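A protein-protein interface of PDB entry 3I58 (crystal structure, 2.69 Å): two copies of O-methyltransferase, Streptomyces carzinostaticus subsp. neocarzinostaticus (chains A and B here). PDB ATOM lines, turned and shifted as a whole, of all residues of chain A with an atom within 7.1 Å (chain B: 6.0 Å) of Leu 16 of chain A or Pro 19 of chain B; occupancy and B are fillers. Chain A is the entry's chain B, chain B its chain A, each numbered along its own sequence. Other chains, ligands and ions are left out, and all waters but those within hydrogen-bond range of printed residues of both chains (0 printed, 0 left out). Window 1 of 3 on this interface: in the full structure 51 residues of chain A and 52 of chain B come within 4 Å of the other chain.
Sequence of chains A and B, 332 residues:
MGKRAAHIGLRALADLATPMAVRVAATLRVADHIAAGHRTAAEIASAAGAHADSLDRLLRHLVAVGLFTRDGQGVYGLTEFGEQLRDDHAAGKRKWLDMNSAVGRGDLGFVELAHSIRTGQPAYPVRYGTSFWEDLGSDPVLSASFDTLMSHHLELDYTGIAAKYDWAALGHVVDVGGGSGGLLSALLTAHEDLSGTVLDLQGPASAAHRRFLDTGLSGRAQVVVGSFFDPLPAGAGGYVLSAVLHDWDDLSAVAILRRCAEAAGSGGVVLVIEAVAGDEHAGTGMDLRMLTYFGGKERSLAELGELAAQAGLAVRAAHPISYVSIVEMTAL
Among the printed residues, pairs that only touch across the chains: Leu 13 of chain A with Pro 19 of chain B (3.6 Å), Ala 14 of chain A with Pro 19 of chain B (3.8 Å), Ala 14 of chain A with Val 22 of chain B (3.95 Å), Asp 15 of chain A with Pro 19 of chain B (3.5 Å), Leu 16 of chain A with Pro 19 of chain B (3.4 Å), Leu 16 of chain A with Arg 23 of chain B (3.7 Å), Leu 16 of chain A with Asp 107 of chain B (3.8 Å), Leu 16 of chain A with Leu 108 of chain B (3.997 Å), Ala 17 of chain A with Phe 110 of chain B (3.7 Å), Pro 19 of chain A with Asp 15 of chain B (3.6 Å), Pro 19 of chain A with Leu 16 of chain B (3.4 Å), Met 20 of chain A with Phe 110 of chain B (3.2 Å), Val 111 of chain A with Met 20 of chain B (3.7 Å), Leu 113 of chain A with Met 20 of chain B (3.9 Å), Leu 113 of chain A with Ala 21 of chain B (3.8 Å) and Leu 113 of chain A with Val 24 of chain B (3.99 Å).
The side-chain carboxylate (OD2) of Asp 15 of chain A sits at hydrogen-bond distance from the backbone NH (N) of Thr 18 of chain A (3.0 Å).
The backbone NH of Ala 17 of chain A is in hydrogen-bond range of the side-chain carboxylate of Asp 15 of chain A.
OD2 of Asp 15 of chain B lies within hydrogen-bond range of N of Thr 18 of chain B, at 2.8 Å.
OD2 of Asp 107 of chain B lies within salt-bridge range of NH2 of Arg 23 of chain B (3.1 Å).
The backbone NH (N) of Ala 17 of chain B lies within hydrogen-bond range of the side-chain carboxylate (OD1) of Asp 15 of chain B (3.1 Å).
Of chain A, only Leu 13 (3.6 Å), Ala 14 (3.8 Å), Asp 15 (3.5 Å) and Leu 16 (3.4 Å) come within 4 Å of Pro 19 of chain B.
Printed residues of chain B within 4 Å of Asp 15 of chain A: Pro 19 (3.5 Å).
Of the printed residues of chain A, Met 20 of chain B touches Val 111 and Leu 113.
Arg 11 of chain A touches none of the printed residues of chain B.
Ala 17 of chain B touches none of the printed residues of chain A.
The backbone carbonyl oxygen of Ala 14 of chain A sits at hydrogen-bond distance from the guanidinium group of Arg 23 of chain B (2.8 Å).
Asp 15 of chain A touches Pro 19 of chain B, and with the chains exchanged Pro 19 of chain A touches Asp 15 of chain B.
Leu 16 of chain A touches Pro 19 of chain B, and with the chains exchanged Pro 19 of chain A touches Leu 16 of chain B.
8 positions are printed for both chains.
Of the 17 pairs that touch across the chains among the printed residues, 4 have their exchanged pair printed and touching as well.
Of the 13 printed residues of chain B, 11 touch a printed residue of chain A.
Hydrophobic or aromatic side chains of chain B that line the printed part of chain A: Leu 16, Pro 19, Met 20, Val 22, Val 24, Leu 108 and Phe 110.
Printed residues of chain A that touch a printed residue of chain B: Leu 13, Ala 14, Asp 15, Leu 16, Ala 17, Pro 19, Met 20, Val 111 and Leu 113.
Along chain A the printed residues that touch a printed residue of chain B span positions 13 to 113.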
ATOM      1  N   ARG A  11       8.377 -31.041  25.597  1.00  0.00           N
ATOM      2  CA  ARG A  11       8.826 -29.678  25.828  1.00  0.00           C
ATOM      3  C   ARG A  11       9.795 -29.590  27.000  1.00  0.00           C
ATOM      4  O   ARG A  11      10.720 -28.777  26.978  1.00  0.00           O
ATOM      5  CB  ARG A  11       7.629 -28.740  26.031  1.00  0.00           C
ATOM      6  CG  ARG A  11       6.791 -28.553  24.768  1.00  0.00           C
ATOM      7  CD  ARG A  11       5.632 -27.599  24.987  1.00  0.00           C
ATOM      8  NE  ARG A  11       6.091 -26.226  25.164  1.00  0.00           N
ATOM      9  CZ  ARG A  11       5.299 -25.203  25.473  1.00  0.00           C
ATOM     10  NH1 ARG A  11       3.994 -25.384  25.642  1.00  0.00           N
ATOM     11  NH2 ARG A  11       5.817 -23.991  25.616  1.00  0.00           N
ATOM     12  N   ALA A  12       9.595 -30.429  28.012  1.00  0.00           N
ATOM     13  CA  ALA A  12      10.478 -30.437  29.170  1.00  0.00           C
ATOM     14  C   ALA A  12      11.828 -30.962  28.708  1.00  0.00           C
ATOM     15  O   ALA A  12      12.884 -30.551  29.185  1.00  0.00           O
ATOM     16  CB  ALA A  12       9.921 -31.332  30.229  1.00  0.00           C
ATOM     17  N   LEU A  13      11.769 -31.888  27.764  1.00  0.00           N
ATOM     18  CA  LEU A  13      12.949 -32.495  27.199  1.00  0.00           C
ATOM     19  C   LEU A  13      13.737 -31.423  26.431  1.00  0.00           C
ATOM     20  O   LEU A  13      14.954 -31.531  26.258  1.00  0.00           O
ATOM     21  CB  LEU A  13      12.501 -33.615  26.266  1.00  0.00           C
ATOM     22  CG  LEU A  13      13.399 -34.813  25.993  1.00  0.00           C
ATOM     23  CD1 LEU A  13      13.792 -35.458  27.296  1.00  0.00           C
ATOM     24  CD2 LEU A  13      12.653 -35.810  25.118  1.00  0.00           C
ATOM     25  N   ALA A  14      13.045 -30.378  25.987  1.00  0.00           N
ATOM     26  CA  ALA A  14      13.678 -29.306  25.230  1.00  0.00           C
ATOM     27  C   ALA A  14      13.950 -28.063  26.072  1.00  0.00           C
ATOM     28  O   ALA A  14      14.311 -27.003  25.541  1.00  0.00           O
ATOM     29  CB  ALA A  14      12.806 -28.936  24.054  1.00  0.00           C
ATOM     30  N   ASP A  15      13.782 -28.198  27.385  1.00  0.00           N
ATOM     31  CA  ASP A  15      13.981 -27.089  28.312  1.00  0.00           C
ATOM     32  C   ASP A  15      15.397 -26.530  28.329  1.00  0.00           C
ATOM     33  O   ASP A  15      16.362 -27.275  28.425  1.00  0.00           O
ATOM     34  CB  ASP A  15      13.614 -27.519  29.725  1.00  0.00           C
ATOM     35  CG  ASP A  15      13.786 -26.401  30.724  1.00  0.00           C
ATOM     36  OD1 ASP A  15      13.126 -25.345  30.569  1.00  0.00           O
ATOM     37  OD2 ASP A  15      14.585 -26.572  31.666  1.00  0.00           O
ATOM     38  N   LEU A  16      15.520 -25.214  28.243  1.00  0.00           N
ATOM     39  CA  LEU A  16      16.829 -24.582  28.273  1.00  0.00           C
ATOM     40  C   LEU A  16      16.988 -23.805  29.569  1.00  0.00           C
ATOM     41  O   LEU A  16      18.098 -23.549  30.013  1.00  0.00           O
ATOM     42  CB  LEU A  16      16.994 -23.642  27.081  1.00  0.00           C
ATOM     43  CG  LEU A  16      16.981 -24.381  25.748  1.00  0.00           C
ATOM     44  CD1 LEU A  16      17.060 -23.402  24.595  1.00  0.00           C
ATOM     45  CD2 LEU A  16      18.147 -25.358  25.714  1.00  0.00           C
ATOM     46  N   ALA A  17      15.867 -23.453  30.184  1.00  0.00           N
ATOM     47  CA  ALA A  17      15.877 -22.687  31.415  1.00  0.00           C
ATOM     48  C   ALA A  17      16.747 -23.302  32.505  1.00  0.00           C
ATOM     49  O   ALA A  17      17.560 -22.626  33.122  1.00  0.00           O
ATOM     50  CB  ALA A  17      14.457 -22.520  31.919  1.00  0.00           C
ATOM     51  N   THR A  18      16.576 -24.593  32.736  1.00  0.00           N
ATOM     52  CA  THR A  18      17.335 -25.265  33.775  1.00  0.00           C
ATOM     53  C   THR A  18      18.804 -25.482  33.407  1.00  0.00           C
ATOM     54  O   THR A  18      19.697 -25.166  34.201  1.00  0.00           O
ATOM     55  CB  THR A  18      16.657 -26.604  34.165  1.00  0.00           C
ATOM     56  OG1 THR A  18      15.394 -26.326  34.781  1.00  0.00           O
ATOM     57  CG2 THR A  18      17.503 -27.367  35.151  1.00  0.00           C
ATOM     58  N   PRO A  19      19.085 -26.021  32.208  1.00  0.00           N
ATOM     59  CA  PRO A  19      20.496 -26.217  31.870  1.00  0.00           C
ATOM     60  C   PRO A  19      21.255 -24.906  32.046  1.00  0.00           C
ATOM     61  O   PRO A  19      22.340 -24.894  32.603  1.00  0.00           O
ATOM     62  CB  PRO A  19      20.445 -26.665  30.409  1.00  0.00           C
ATOM     63  CG  PRO A  19      19.139 -27.367  30.319  1.00  0.00           C
ATOM     64  CD  PRO A  19      18.216 -26.466  31.106  1.00  0.00           C
ATOM     65  N   MET A  20      20.673 -23.805  31.579  1.00  0.00           N
ATOM     66  CA  MET A  20      21.310 -22.500  31.700  1.00  0.00           C
ATOM     67  C   MET A  20      21.365 -22.020  33.143  1.00  0.00           C
ATOM     68  O   MET A  20      22.339 -21.398  33.552  1.00  0.00           O
ATOM     69  CB  MET A  20      20.585 -21.439  30.865  1.00  0.00           C
ATOM     70  CG  MET A  20      20.761 -21.550  29.365  1.00  0.00           C
ATOM     71  SD  MET A  20      22.436 -21.899  28.833  1.00  0.00           S
ATOM     72  CE  MET A  20      23.313 -20.612  29.627  1.00  0.00           C
ATOM     73  N   ALA A  21      20.315 -22.294  33.910  1.00  0.00           N
ATOM     74  CA  ALA A  21      20.272 -21.884  35.303  1.00  0.00           C
ATOM     75  C   ALA A  21      21.392 -22.559  36.089  1.00  0.00           C
ATOM     76  O   ALA A  21      22.005 -21.941  36.963  1.00  0.00           O
ATOM     77  CB  ALA A  21      18.936 -22.234  35.910  1.00  0.00           C
ATOM     78  N   VAL A  22      21.654 -23.826  35.794  1.00  0.00           N
ATOM     79  CA  VAL A  22      22.721 -24.537  36.490  1.00  0.00           C
ATOM     80  C   VAL A  22      24.055 -23.923  36.063  1.00  0.00           C
ATOM     81  O   VAL A  22      24.899 -23.614  36.898  1.00  0.00           O
ATOM     82  CB  VAL A  22      22.729 -26.056  36.148  1.00  0.00           C
ATOM     83  CG1 VAL A  22      24.016 -26.702  36.645  1.00  0.00           C
ATOM     84  CG2 VAL A  22      21.529 -26.737  36.780  1.00  0.00           C
ATOM     85  N   HIS A  61      14.263 -21.208  41.315  1.00  0.00           N
ATOM     86  CA  HIS A  61      14.095 -22.198  40.260  1.00  0.00           C
ATOM     87  C   HIS A  61      15.024 -23.371  40.539  1.00  0.00           C
ATOM     88  O   HIS A  61      14.693 -24.523  40.261  1.00  0.00           O
ATOM     89  CB  HIS A  61      14.416 -21.605  38.883  1.00  0.00           C
ATOM     90  CG  HIS A  61      14.429 -22.620  37.783  1.00  0.00           C
ATOM     91  ND1 HIS A  61      13.285 -23.247  37.333  1.00  0.00           N
ATOM     92  CD2 HIS A  61      15.457 -23.185  37.102  1.00  0.00           C
ATOM     93  CE1 HIS A  61      13.610 -24.158  36.431  1.00  0.00           C
ATOM     94  NE2 HIS A  61      14.922 -24.141  36.273  1.00  0.00           N
ATOM     95  N   VAL A 111      23.635 -23.655  20.862  1.00  0.00           N
ATOM     96  CA  VAL A 111      22.476 -22.889  20.400  1.00  0.00           C
ATOM     97  C   VAL A 111      22.513 -22.699  18.891  1.00  0.00           C
ATOM     98  O   VAL A 111      21.555 -22.211  18.311  1.00  0.00           O
ATOM     99  CB  VAL A 111      22.344 -21.477  21.052  1.00  0.00           C
ATOM    100  CG1 VAL A 111      22.093 -21.613  22.534  1.00  0.00           C
ATOM    101  CG2 VAL A 111      23.590 -20.633  20.788  1.00  0.00           C
ATOM    102  N   LEU A 113      23.381 -25.364  16.901  1.00  0.00           N
ATOM    103  CA  LEU A 113      23.414 -26.736  16.403  1.00  0.00           C
ATOM    104  C   LEU A 113      22.808 -26.817  15.001  1.00  0.00           C
ATOM    105  O   LEU A 113      23.352 -27.481  14.122  1.00  0.00           O
ATOM    106  CB  LEU A 113      22.630 -27.660  17.337  1.00  0.00           C
ATOM    107  CG  LEU A 113      23.123 -29.090  17.616  1.00  0.00           C
ATOM    108  CD1 LEU A 113      21.930 -29.962  17.951  1.00  0.00           C
ATOM    109  CD2 LEU A 113      23.875 -29.662  16.430  1.00  0.00           C
ATOM    110  N   ASP B  15      22.987 -30.341  30.616  1.00  0.00           N
ATOM    111  CA  ASP B  15      23.200 -30.698  29.212  1.00  0.00           C
ATOM    112  C   ASP B  15      22.427 -29.818  28.241  1.00  0.00           C
ATOM    113  O   ASP B  15      21.250 -29.540  28.443  1.00  0.00           O
ATOM    114  CB  ASP B  15      22.798 -32.146  28.951  1.00  0.00           C
ATOM    115  CG  ASP B  15      22.897 -32.516  27.477  1.00  0.00           C
ATOM    116  OD1 ASP B  15      24.016 -32.483  26.914  1.00  0.00           O
ATOM    117  OD2 ASP B  15      21.853 -32.838  26.877  1.00  0.00           O
ATOM    118  N   LEU B  16      23.090 -29.384  27.180  1.00  0.00           N
ATOM    119  CA  LEU B  16      22.441 -28.557  26.181  1.00  0.00           C
ATOM    120  C   LEU B  16      22.297 -29.337  24.880  1.00  0.00           C
ATOM    121  O   LEU B  16      21.504 -28.982  24.026  1.00  0.00           O
ATOM    122  CB  LEU B  16      23.244 -27.278  25.946  1.00  0.00           C
ATOM    123  CG  LEU B  16      23.271 -26.301  27.122  1.00  0.00           C
ATOM    124  CD1 LEU B  16      24.138 -25.104  26.781  1.00  0.00           C
ATOM    125  CD2 LEU B  16      21.858 -25.846  27.444  1.00  0.00           C
ATOM    126  N   ALA B  17      23.052 -30.417  24.743  1.00  0.00           N
ATOM    127  CA  ALA B  17      23.002 -31.230  23.540  1.00  0.00           C
ATOM    128  C   ALA B  17      21.611 -31.783  23.238  1.00  0.00           C
ATOM    129  O   ALA B  17      21.145 -31.736  22.108  1.00  0.00           O
ATOM    130  CB  ALA B  17      23.992 -32.372  23.651  1.00  0.00           C
ATOM    131  N   THR B  18      20.941 -32.308  24.248  1.00  0.00           N
ATOM    132  CA  THR B  18      19.622 -32.870  24.021  1.00  0.00           C
ATOM    133  C   THR B  18      18.536 -31.818  23.778  1.00  0.00           C
ATOM    134  O   THR B  18      17.752 -31.938  22.831  1.00  0.00           O
ATOM    135  CB  THR B  18      19.239 -33.801  25.176  1.00  0.00           C
ATOM    136  OG1 THR B  18      20.168 -34.896  25.205  1.00  0.00           O
ATOM    137  CG2 THR B  18      17.843 -34.348  24.984  1.00  0.00           C
ATOM    138  N   PRO B  19      18.472 -30.771  24.620  1.00  0.00           N
ATOM    139  CA  PRO B  19      17.442 -29.751  24.398  1.00  0.00           C
ATOM    140  C   PRO B  19      17.562 -29.188  22.984  1.00  0.00           C
ATOM    141  O   PRO B  19      16.570 -29.071  22.284  1.00  0.00           O
ATOM    142  CB  PRO B  19      17.757 -28.705  25.463  1.00  0.00           C
ATOM    143  CG  PRO B  19      18.347 -29.511  26.555  1.00  0.00           C
ATOM    144  CD  PRO B  19      19.254 -30.466  25.826  1.00  0.00           C
ATOM    145  N   MET B  20      18.783 -28.852  22.572  1.00  0.00           N
ATOM    146  CA  MET B  20      19.027 -28.312  21.238  1.00  0.00           C
ATOM    147  C   MET B  20      18.772 -29.332  20.138  1.00  0.00           C
ATOM    148  O   MET B  20      18.289 -28.978  19.066  1.00  0.00           O
ATOM    149  CB  MET B  20      20.461 -27.792  21.111  1.00  0.00           C
ATOM    150  CG  MET B  20      20.736 -26.527  21.893  1.00  0.00           C
ATOM    151  SD  MET B  20      19.430 -25.305  21.695  1.00  0.00           S
ATOM    152  CE  MET B  20      19.523 -25.000  19.963  1.00  0.00           C
ATOM    153  N   ALA B  21      19.107 -30.591  20.394  1.00  0.00           N
ATOM    154  CA  ALA B  21      18.884 -31.643  19.413  1.00  0.00           C
ATOM    155  C   ALA B  21      17.390 -31.820  19.163  1.00  0.00           C
ATOM    156  O   ALA B  21      16.975 -32.076  18.034  1.00  0.00           O
ATOM    157  CB  ALA B  21      19.475 -32.945  19.893  1.00  0.00           C
ATOM    158  N   VAL B  22      16.583 -31.690  20.210  1.00  0.00           N
ATOM    159  CA  VAL B  22      15.139 -31.831  20.063  1.00  0.00           C
ATOM    160  C   VAL B  22      14.587 -30.639  19.285  1.00  0.00           C
ATOM    161  O   VAL B  22      13.770 -30.804  18.382  1.00  0.00           O
ATOM    162  CB  VAL B  22      14.423 -31.912  21.437  1.00  0.00           C
ATOM    163  CG1 VAL B  22      12.920 -31.732  21.266  1.00  0.00           C
ATOM    164  CG2 VAL B  22      14.709 -33.251  22.084  1.00  0.00           C
ATOM    165  N   ARG B  23      15.041 -29.439  19.630  1.00  0.00           N
ATOM    166  CA  ARG B  23      14.573 -28.249  18.946  1.00  0.00           C
ATOM    167  C   ARG B  23      14.964 -28.281  17.476  1.00  0.00           C
ATOM    168  O   ARG B  23      14.199 -27.849  16.626  1.00  0.00           O
ATOM    169  CB  ARG B  23      15.114 -26.993  19.634  1.00  0.00           C
ATOM    170  CG  ARG B  23      14.455 -26.738  20.980  1.00  0.00           C
ATOM    171  CD  ARG B  23      15.193 -25.730  21.830  1.00  0.00           C
ATOM    172  NE  ARG B  23      14.539 -25.602  23.126  1.00  0.00           N
ATOM    173  CZ  ARG B  23      13.524 -24.782  23.378  1.00  0.00           C
ATOM    174  NH1 ARG B  23      13.054 -24.002  22.416  1.00  0.00           N
ATOM    175  NH2 ARG B  23      12.968 -24.752  24.585  1.00  0.00           N
ATOM    176  N   VAL B  24      16.151 -28.792  17.170  1.00  0.00           N
ATOM    177  CA  VAL B  24      16.572 -28.873  15.778  1.00  0.00           C
ATOM    178  C   VAL B  24      15.702 -29.885  15.020  1.00  0.00           C
ATOM    179  O   VAL B  24      15.312 -29.636  13.878  1.00  0.00           O
ATOM    180  CB  VAL B  24      18.070 -29.252  15.656  1.00  0.00           C
ATOM    181  CG1 VAL B  24      18.388 -29.740  14.241  1.00  0.00           C
ATOM    182  CG2 VAL B  24      18.917 -28.046  15.939  1.00  0.00           C
ATOM    183  N   ASP B 107      13.300 -18.497  23.168  1.00  0.00           N
ATOM    184  CA  ASP B 107      13.844 -19.421  24.151  1.00  0.00           C
ATOM    185  C   ASP B 107      15.356 -19.570  24.021  1.00  0.00           C
ATOM    186  O   ASP B 107      16.044 -19.809  25.009  1.00  0.00           O
ATOM    187  CB  ASP B 107      13.160 -20.785  24.049  1.00  0.00           C
ATOM    188  CG  ASP B 107      12.009 -20.935  25.024  1.00  0.00           C
ATOM    189  OD1 ASP B 107      11.478 -19.905  25.485  1.00  0.00           O
ATOM    190  OD2 ASP B 107      11.633 -22.082  25.331  1.00  0.00           O
ATOM    191  N   LEU B 108      15.879 -19.426  22.807  1.00  0.00           N
ATOM    192  CA  LEU B 108      17.314 -19.523  22.616  1.00  0.00           C
ATOM    193  C   LEU B 108      17.980 -18.351  23.330  1.00  0.00           C
ATOM    194  O   LEU B 108      19.194 -18.315  23.481  1.00  0.00           O
ATOM    195  CB  LEU B 108      17.674 -19.506  21.132  1.00  0.00           C
ATOM    196  CG  LEU B 108      17.084 -20.625  20.274  1.00  0.00           C
ATOM    197  CD1 LEU B 108      17.668 -20.517  18.868  1.00  0.00           C
ATOM    198  CD2 LEU B 108      17.392 -21.990  20.871  1.00  0.00           C
ATOM    199  N   PHE B 110      17.877 -17.839  26.297  1.00  0.00           N
ATOM    200  CA  PHE B 110      18.355 -18.328  27.583  1.00  0.00           C
ATOM    201  C   PHE B 110      19.854 -18.484  27.585  1.00  0.00           C
ATOM    202  O   PHE B 110      20.482 -18.447  28.645  1.00  0.00           O
ATOM    203  CB  PHE B 110      17.722 -19.671  27.942  1.00  0.00           C
ATOM    204  CG  PHE B 110      16.437 -19.548  28.710  1.00  0.00           C
ATOM    205  CD1 PHE B 110      15.226 -19.913  28.133  1.00  0.00           C
ATOM    206  CD2 PHE B 110      16.437 -19.052  30.010  1.00  0.00           C
ATOM    207  CE1 PHE B 110      14.038 -19.784  28.836  1.00  0.00           C
ATOM    208  CE2 PHE B 110      15.248 -18.919  30.726  1.00  0.00           C
ATOM    209  CZ  PHE B 110      14.047 -19.284  30.137  1.00  0.00           C
